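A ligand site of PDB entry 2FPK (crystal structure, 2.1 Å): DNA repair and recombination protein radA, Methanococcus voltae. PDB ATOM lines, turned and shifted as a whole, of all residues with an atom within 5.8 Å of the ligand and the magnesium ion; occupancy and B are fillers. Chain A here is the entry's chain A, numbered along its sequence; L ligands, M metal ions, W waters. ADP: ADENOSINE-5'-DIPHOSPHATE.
N6 of the ligand sits close to NH2 of Arg 158 (3.3 Å). Residues that only touch the ligand: Val 106, Phe 107, Ser 109, Arg 296, Ile 315, Thr 316 and Glu 317. Hydrophobic or aromatic side chains within 4 Å of the ligand: Phe 107 and Ile 315. Within 4 Å of the ligand: Val 106, Phe 107, Gly 108, Ser 109, Gly 110, Lys 111, Thr 112, Gln 113, Arg 158, Gln 161, Arg 296, Ile 315, Thr 316 and Glu 317. The nearest printed residue that does not touch the ligand is Gln 257 (4.05 Å).
Of the 23 residues printed, 1 comes within 4 Å of the magnesium ion. The nearest printed residue that does not touch the magnesium ion is Asp 211 (4.1 Å).
An oxygen (O2B) of the ligand sits at hydrogen-bond distance from the backbone NH of Lys 111. The backbone NH (N) of Gln 113 lies within hydrogen-bond range of an oxygen (O1A) of the ligand (2.8 Å). The side-chain amide oxygen (OE1) of Gln 161 sits at hydrogen-bond distance from a nitrogen (N6) of the ligand (2.9 Å). An oxygen (O2B) of the ligand lies within salt-bridge range of the side-chain amino group (NZ) of Lys 111 (2.6 Å). N of Thr 112 is in hydrogen-bond range of O1A of the ligand (2.8 Å). The backbone NH of Gly 110 is in hydrogen-bond range of an oxygen (O2B) of the ligand (3.1 Å). The backbone NH (N) of Gly 108 sits at hydrogen-bond distance from an oxygen (O3B) of the ligand (2.6 Å).
Water W1 bridges NE2 of Gln 161 (2.7 Å) and N6 of the ligand (3.1 Å).
The side-chain amide oxygen (OE1) of Gln 257 lies close to the backbone NH (N) of Phe 107 (3.2 Å). The side-chain amide oxygen of Gln 113 sits at hydrogen-bond distance from the guanidinium group of Arg 158 (2.8 Å). OE1 of Gln 161 lies within hydrogen-bond range of NH2 of Arg 158 (2.8 Å). N of Lys 318 lies close to OG1 of Thr 316, at 3.1 Å. The backbone carbonyl oxygen of Glu 317 sits at hydrogen-bond distance from the guanidinium group of Arg 158, at 3.0 Å. The backbone carbonyl oxygen (O) of Val 106 sits at hydrogen-bond distance from the side-chain hydroxyl (OG) of Ser 109 (2.8 Å). NZ of Lys 111 sits close to NE2 of Gln 257 (2.8 Å). NE of Arg 296 sits close to O of Ser 109 (3.2 Å).
The magnesium ion is bound by the side-chain hydroxyl of Thr 112 (1.9 Å), an oxygen (O1B) of the ligand (2.0 Å), water W3 (2.0 Å), water W4 (2.0 Å), water W6 (2.1 Å) and water W5 (2.2 Å). The magnesium ion has six donor atoms within binding distance.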
ATOM      1  N   GLY A 105      17.518  35.693  16.383  1.00  0.00           N
ATOM      2  CA  GLY A 105      16.396  35.131  15.654  1.00  0.00           C
ATOM      3  C   GLY A 105      15.101  35.823  15.990  1.00  0.00           C
ATOM      4  O   GLY A 105      15.027  36.600  16.943  1.00  0.00           O
ATOM      5  N   VAL A 106      14.064  35.547  15.205  1.00  0.00           N
ATOM      6  CA  VAL A 106      12.765  36.162  15.449  1.00  0.00           C
ATOM      7  C   VAL A 106      12.151  35.597  16.724  1.00  0.00           C
ATOM      8  O   VAL A 106      12.651  34.614  17.275  1.00  0.00           O
ATOM      9  CB  VAL A 106      11.795  35.898  14.273  1.00  0.00           C
ATOM     10  CG1 VAL A 106      12.388  36.441  12.965  1.00  0.00           C
ATOM     11  CG2 VAL A 106      11.490  34.404  14.163  1.00  0.00           C
ATOM     12  N   PHE A 107      11.080  36.229  17.181  1.00  0.00           N
ATOM     13  CA  PHE A 107      10.419  35.773  18.389  1.00  0.00           C
ATOM     14  C   PHE A 107       9.925  34.345  18.186  1.00  0.00           C
ATOM     15  O   PHE A 107       9.412  34.001  17.125  1.00  0.00           O
ATOM     16  CB  PHE A 107       9.243  36.678  18.764  1.00  0.00           C
ATOM     17  CG  PHE A 107       8.819  36.560  20.204  1.00  0.00           C
ATOM     18  CD1 PHE A 107       8.718  37.697  21.003  1.00  0.00           C
ATOM     19  CD2 PHE A 107       8.558  35.323  20.777  1.00  0.00           C
ATOM     20  CE1 PHE A 107       8.353  37.600  22.350  1.00  0.00           C
ATOM     21  CE2 PHE A 107       8.195  35.204  22.125  1.00  0.00           C
ATOM     22  CZ  PHE A 107       8.094  36.350  22.913  1.00  0.00           C
ATOM     23  N   GLY A 108      10.106  33.524  19.216  1.00  0.00           N
ATOM     24  CA  GLY A 108       9.648  32.160  19.166  1.00  0.00           C
ATOM     25  C   GLY A 108      10.593  31.181  18.508  1.00  0.00           C
ATOM     26  O   GLY A 108      10.309  29.995  18.467  1.00  0.00           O
ATOM     27  N   SER A 109      11.711  31.659  17.984  1.00  0.00           N
ATOM     28  CA  SER A 109      12.648  30.756  17.313  1.00  0.00           C
ATOM     29  C   SER A 109      13.379  29.788  18.235  1.00  0.00           C
ATOM     30  O   SER A 109      13.905  28.771  17.771  1.00  0.00           O
ATOM     31  CB  SER A 109      13.658  31.559  16.471  1.00  0.00           C
ATOM     32  OG  SER A 109      14.393  32.465  17.280  1.00  0.00           O
ATOM     33  N   GLY A 110      13.435  30.096  19.538  1.00  0.00           N
ATOM     34  CA  GLY A 110      14.084  29.192  20.476  1.00  0.00           C
ATOM     35  C   GLY A 110      15.286  29.684  21.256  1.00  0.00           C
ATOM     36  O   GLY A 110      16.001  28.886  21.881  1.00  0.00           O
ATOM     37  N   LYS A 111      15.529  30.999  21.244  1.00  0.00           N
ATOM     38  CA  LYS A 111      16.669  31.561  21.938  1.00  0.00           C
ATOM     39  C   LYS A 111      16.627  31.310  23.455  1.00  0.00           C
ATOM     40  O   LYS A 111      17.621  30.897  24.055  1.00  0.00           O
ATOM     41  CB  LYS A 111      16.723  33.073  21.667  1.00  0.00           C
ATOM     42  CG  LYS A 111      16.763  33.435  20.206  1.00  0.00           C
ATOM     43  CD  LYS A 111      16.863  34.951  20.024  1.00  0.00           C
ATOM     44  CE  LYS A 111      15.570  35.625  20.462  1.00  0.00           C
ATOM     45  NZ  LYS A 111      14.448  35.131  19.633  1.00  0.00           N
ATOM     46  N   THR A 112      15.483  31.557  24.062  1.00  0.00           N
ATOM     47  CA  THR A 112      15.343  31.367  25.497  1.00  0.00           C
ATOM     48  C   THR A 112      15.438  29.885  25.854  1.00  0.00           C
ATOM     49  O   THR A 112      15.977  29.524  26.910  1.00  0.00           O
ATOM     50  CB  THR A 112      13.995  31.969  25.963  1.00  0.00           C
ATOM     51  OG1 THR A 112      14.040  33.397  25.753  1.00  0.00           O
ATOM     52  CG2 THR A 112      13.748  31.684  27.456  1.00  0.00           C
ATOM     53  N   GLN A 113      14.938  29.038  24.972  1.00  0.00           N
ATOM     54  CA  GLN A 113      15.005  27.596  25.192  1.00  0.00           C
ATOM     55  C   GLN A 113      16.467  27.144  25.265  1.00  0.00           C
ATOM     56  O   GLN A 113      16.853  26.407  26.163  1.00  0.00           O
ATOM     57  CB  GLN A 113      14.289  26.857  24.048  1.00  0.00           C
ATOM     58  CG  GLN A 113      12.771  27.137  23.991  1.00  0.00           C
ATOM     59  CD  GLN A 113      12.108  26.949  25.345  1.00  0.00           C
ATOM     60  OE1 GLN A 113      12.021  25.823  25.861  1.00  0.00           O
ATOM     61  NE2 GLN A 113      11.641  28.050  25.939  1.00  0.00           N
ATOM     62  N   ILE A 114      17.292  27.622  24.339  1.00  0.00           N
ATOM     63  CA  ILE A 114      18.706  27.248  24.367  1.00  0.00           C
ATOM     64  C   ILE A 114      19.374  27.752  25.629  1.00  0.00           C
ATOM     65  O   ILE A 114      20.253  27.091  26.182  1.00  0.00           O
ATOM     66  CB  ILE A 114      19.430  27.776  23.113  1.00  0.00           C
ATOM     67  CG1 ILE A 114      18.726  27.219  21.865  1.00  0.00           C
ATOM     68  CG2 ILE A 114      20.894  27.358  23.131  1.00  0.00           C
ATOM     69  CD1 ILE A 114      19.299  27.687  20.546  1.00  0.00           C
ATOM     70  N   GLU A 151      13.906  39.915  29.926  1.00  0.00           N
ATOM     71  CA  GLU A 151      12.523  39.900  29.475  1.00  0.00           C
ATOM     72  C   GLU A 151      11.542  39.415  30.535  1.00  0.00           C
ATOM     73  O   GLU A 151      10.352  39.709  30.473  1.00  0.00           O
ATOM     74  CB  GLU A 151      12.386  38.970  28.259  1.00  0.00           C
ATOM     75  CG  GLU A 151      13.557  38.970  27.288  1.00  0.00           C
ATOM     76  CD  GLU A 151      13.489  40.126  26.317  1.00  0.00           C
ATOM     77  OE1 GLU A 151      14.132  40.036  25.251  1.00  0.00           O
ATOM     78  OE2 GLU A 151      12.786  41.116  26.637  1.00  0.00           O
ATOM     79  N   THR A 153      11.385  36.106  31.139  1.00  0.00           N
ATOM     80  CA  THR A 153      10.958  34.802  30.646  1.00  0.00           C
ATOM     81  C   THR A 153      11.694  33.605  31.256  1.00  0.00           C
ATOM     82  O   THR A 153      11.548  32.473  30.782  1.00  0.00           O
ATOM     83  CB  THR A 153      11.040  34.710  29.101  1.00  0.00           C
ATOM     84  OG1 THR A 153      12.282  35.260  28.651  1.00  0.00           O
ATOM     85  CG2 THR A 153       9.877  35.468  28.465  1.00  0.00           C
ATOM     86  N   ARG A 158      10.398  25.116  33.454  1.00  0.00           N
ATOM     87  CA  ARG A 158      11.026  24.617  32.242  1.00  0.00           C
ATOM     88  C   ARG A 158      12.381  24.007  32.573  1.00  0.00           C
ATOM     89  O   ARG A 158      12.775  23.006  31.977  1.00  0.00           O
ATOM     90  CB  ARG A 158      11.193  25.743  31.220  1.00  0.00           C
ATOM     91  CG  ARG A 158      11.708  25.279  29.863  1.00  0.00           C
ATOM     92  CD  ARG A 158      10.874  24.125  29.271  1.00  0.00           C
ATOM     93  NE  ARG A 158      11.138  23.981  27.837  1.00  0.00           N
ATOM     94  CZ  ARG A 158      10.990  22.857  27.139  1.00  0.00           C
ATOM     95  NH1 ARG A 158      11.255  22.846  25.831  1.00  0.00           N
ATOM     96  NH2 ARG A 158      10.584  21.739  27.719  1.00  0.00           N
ATOM     97  N   GLN A 161      11.725  20.580  34.100  1.00  0.00           N
ATOM     98  CA  GLN A 161      11.281  19.652  33.067  1.00  0.00           C
ATOM     99  C   GLN A 161      12.419  19.113  32.208  1.00  0.00           C
ATOM    100  O   GLN A 161      12.493  17.912  31.954  1.00  0.00           O
ATOM    101  CB  GLN A 161      10.231  20.334  32.185  1.00  0.00           C
ATOM    102  CG  GLN A 161       9.738  19.475  31.039  1.00  0.00           C
ATOM    103  CD  GLN A 161       8.636  20.151  30.242  1.00  0.00           C
ATOM    104  OE1 GLN A 161       8.794  21.282  29.763  1.00  0.00           O
ATOM    105  NE2 GLN A 161       7.506  19.461  30.089  1.00  0.00           N
ATOM    106  N   ASP A 211      19.835  37.129  28.507  1.00  0.00           N
ATOM    107  CA  ASP A 211      18.629  36.973  27.696  1.00  0.00           C
ATOM    108  C   ASP A 211      17.640  38.094  28.020  1.00  0.00           C
ATOM    109  O   ASP A 211      16.928  38.024  29.006  1.00  0.00           O
ATOM    110  CB  ASP A 211      18.037  35.592  27.991  1.00  0.00           C
ATOM    111  CG  ASP A 211      16.868  35.248  27.118  1.00  0.00           C
ATOM    112  OD1 ASP A 211      16.754  35.798  26.006  1.00  0.00           O
ATOM    113  OD2 ASP A 211      16.047  34.401  27.539  1.00  0.00           O
ATOM    114  N   THR A 255      21.392  36.412  23.747  1.00  0.00           N
ATOM    115  CA  THR A 255      20.352  36.274  22.739  1.00  0.00           C
ATOM    116  C   THR A 255      20.073  37.640  22.145  1.00  0.00           C
ATOM    117  O   THR A 255      20.329  38.665  22.773  1.00  0.00           O
ATOM    118  CB  THR A 255      19.062  35.662  23.321  1.00  0.00           C
ATOM    119  OG1 THR A 255      18.493  36.557  24.287  1.00  0.00           O
ATOM    120  CG2 THR A 255      19.384  34.324  24.003  1.00  0.00           C
ATOM    121  N   GLN A 257      16.998  39.452  19.611  1.00  0.00           N
ATOM    122  CA  GLN A 257      15.758  39.397  18.851  1.00  0.00           C
ATOM    123  C   GLN A 257      15.913  40.212  17.563  1.00  0.00           C
ATOM    124  O   GLN A 257      16.326  41.354  17.601  1.00  0.00           O
ATOM    125  CB  GLN A 257      14.617  39.975  19.687  1.00  0.00           C
ATOM    126  CG  GLN A 257      13.221  39.703  19.159  1.00  0.00           C
ATOM    127  CD  GLN A 257      12.590  38.457  19.760  1.00  0.00           C
ATOM    128  OE1 GLN A 257      11.385  38.246  19.640  1.00  0.00           O
ATOM    129  NE2 GLN A 257      13.394  37.625  20.418  1.00  0.00           N
ATOM    130  N   LYS A 290      12.548  29.190  12.984  1.00  0.00           N
ATOM    131  CA  LYS A 290      11.637  28.093  13.258  1.00  0.00           C
ATOM    132  C   LYS A 290      11.369  27.330  11.979  1.00  0.00           C
ATOM    133  O   LYS A 290      11.120  27.926  10.935  1.00  0.00           O
ATOM    134  CB  LYS A 290      10.330  28.623  13.854  1.00  0.00           C
ATOM    135  CG  LYS A 290       9.473  27.569  14.546  1.00  0.00           C
ATOM    136  CD  LYS A 290       8.261  28.204  15.224  1.00  0.00           C
ATOM    137  CE  LYS A 290       7.385  27.166  15.929  1.00  0.00           C
ATOM    138  NZ  LYS A 290       6.834  26.131  14.998  1.00  0.00           N
ATOM    139  N   ARG A 296      13.852  23.285  14.085  1.00  0.00           N
ATOM    140  CA  ARG A 296      14.532  24.558  14.279  1.00  0.00           C
ATOM    141  C   ARG A 296      15.826  24.476  13.479  1.00  0.00           C
ATOM    142  O   ARG A 296      16.445  23.420  13.396  1.00  0.00           O
ATOM    143  CB  ARG A 296      14.858  24.778  15.760  1.00  0.00           C
ATOM    144  CG  ARG A 296      13.639  24.931  16.653  1.00  0.00           C
ATOM    145  CD  ARG A 296      12.875  26.206  16.331  1.00  0.00           C
ATOM    146  NE  ARG A 296      11.797  26.444  17.272  1.00  0.00           N
ATOM    147  CZ  ARG A 296      10.688  25.712  17.352  1.00  0.00           C
ATOM    148  NH1 ARG A 296      10.506  24.695  16.514  1.00  0.00           N
ATOM    149  NH2 ARG A 296       9.774  26.004  18.263  1.00  0.00           N
ATOM    150  N   ILE A 315      12.813  21.280  19.433  1.00  0.00           N
ATOM    151  CA  ILE A 315      12.483  21.674  20.791  1.00  0.00           C
ATOM    152  C   ILE A 315      11.235  20.901  21.180  1.00  0.00           C
ATOM    153  O   ILE A 315      10.180  21.031  20.558  1.00  0.00           O
ATOM    154  CB  ILE A 315      12.224  23.185  20.878  1.00  0.00           C
ATOM    155  CG1 ILE A 315      13.475  23.976  20.457  1.00  0.00           C
ATOM    156  CG2 ILE A 315      11.824  23.556  22.302  1.00  0.00           C
ATOM    157  CD1 ILE A 315      13.291  25.496  20.459  1.00  0.00           C
ATOM    158  N   THR A 316      11.362  20.082  22.206  1.00  0.00           N
ATOM    159  CA  THR A 316      10.252  19.261  22.686  1.00  0.00           C
ATOM    160  C   THR A 316      10.142  19.478  24.185  1.00  0.00           C
ATOM    161  O   THR A 316      10.790  20.367  24.738  1.00  0.00           O
ATOM    162  CB  THR A 316      10.533  17.771  22.419  1.00  0.00           C
ATOM    163  OG1 THR A 316      11.622  17.347  23.245  1.00  0.00           O
ATOM    164  CG2 THR A 316      10.918  17.545  20.945  1.00  0.00           C
ATOM    165  N   GLU A 317       9.345  18.659  24.864  1.00  0.00           N
ATOM    166  CA  GLU A 317       9.200  18.802  26.301  1.00  0.00           C
ATOM    167  C   GLU A 317      10.509  18.446  26.991  1.00  0.00           C
ATOM    168  O   GLU A 317      10.730  18.797  28.142  1.00  0.00           O
ATOM    169  CB  GLU A 317       8.059  17.916  26.831  1.00  0.00           C
ATOM    170  CG  GLU A 317       7.503  16.901  25.853  1.00  0.00           C
ATOM    171  CD  GLU A 317       8.441  15.740  25.582  1.00  0.00           C
ATOM    172  OE1 GLU A 317       8.862  15.069  26.554  1.00  0.00           O
ATOM    173  OE2 GLU A 317       8.748  15.492  24.403  1.00  0.00           O
ATOM    174  N   LYS A 318      11.395  17.760  26.262  1.00  0.00           N
ATOM    175  CA  LYS A 318      12.678  17.378  26.828  1.00  0.00           C
ATOM    176  C   LYS A 318      13.706  18.493  26.668  1.00  0.00           C
ATOM    177  O   LYS A 318      14.794  18.427  27.240  1.00  0.00           O
ATOM    178  CB  LYS A 318      13.204  16.117  26.139  1.00  0.00           C
ATOM    179  CG  LYS A 318      12.364  14.873  26.380  1.00  0.00           C
ATOM    180  CD  LYS A 318      13.093  13.634  25.892  1.00  0.00           C
ATOM    181  CE  LYS A 318      12.320  12.356  26.210  1.00  0.00           C
ATOM    182  NZ  LYS A 318      11.054  12.294  25.436  1.00  0.00           N
HETATM  183  PB  ADP L   1      12.429  33.042  21.725  1.00  0.00           P
HETATM  184  O1B ADP L   1      13.020  33.285  23.070  1.00  0.00           O
HETATM  185  O2B ADP L   1      13.504  32.962  20.717  1.00  0.00           O
HETATM  186  O3B ADP L   1      11.422  34.220  21.360  1.00  0.00           O
HETATM  187  PA  ADP L   1      11.651  30.647  22.968  1.00  0.00           P
HETATM  188  O1A ADP L   1      13.091  30.300  23.332  1.00  0.00           O
HETATM  189  O2A ADP L   1      10.989  31.279  24.130  1.00  0.00           O
HETATM  190  O3A ADP L   1      11.628  31.651  21.705  1.00  0.00           O
HETATM  191  O5' ADP L   1      10.867  29.261  22.509  1.00  0.00           O
HETATM  192  C5' ADP L   1       9.357  29.144  22.430  1.00  0.00           C
HETATM  193  C4' ADP L   1       9.059  27.949  21.924  1.00  0.00           C
HETATM  194  O4' ADP L   1       9.587  26.899  22.811  1.00  0.00           O
HETATM  195  C3' ADP L   1       7.520  27.687  21.984  1.00  0.00           C
HETATM  196  O3' ADP L   1       6.736  28.484  21.202  1.00  0.00           O
HETATM  197  C2' ADP L   1       7.383  26.143  22.146  1.00  0.00           C
HETATM  198  O2' ADP L   1       7.244  25.542  20.743  1.00  0.00           O
HETATM  199  C1' ADP L   1       8.732  25.719  22.722  1.00  0.00           C
HETATM  200  N9  ADP L   1       8.488  25.243  23.958  1.00  0.00           N
HETATM  201  C8  ADP L   1       8.576  25.952  25.169  1.00  0.00           C
HETATM  202  N7  ADP L   1       8.268  25.173  26.148  1.00  0.00           N
HETATM  203  C5  ADP L   1       7.971  23.953  25.676  1.00  0.00           C
HETATM  204  C6  ADP L   1       7.585  22.765  26.265  1.00  0.00           C
HETATM  205  N6  ADP L   1       7.434  22.701  27.618  1.00  0.00           N
HETATM  206  N1  ADP L   1       7.347  21.640  25.455  1.00  0.00           N
HETATM  207  C2  ADP L   1       7.493  21.705  24.032  1.00  0.00           C
HETATM  208  N3  ADP L   1       7.871  22.867  23.416  1.00  0.00           N
HETATM  209  C4  ADP L   1       8.104  23.973  24.291  1.00  0.00           C
HETATM  210 MG    MG M   1      13.080  34.581  24.597  1.00  0.00          MG
HETATM  211  O   HOH W   1       5.554  20.406  28.482  1.00  0.00           O
HETATM  212  O   HOH W   2       8.189  32.451  23.825  1.00  0.00           O
HETATM  213  O   HOH W   3      11.368  33.673  25.146  1.00  0.00           O
HETATM  214  O   HOH W   4      12.532  35.987  25.969  1.00  0.00           O
HETATM  215  O   HOH W   5      14.828  35.809  24.170  1.00  0.00           O
HETATM  216  O   HOH W   6      11.713  35.671  23.372  1.00  0.00           O
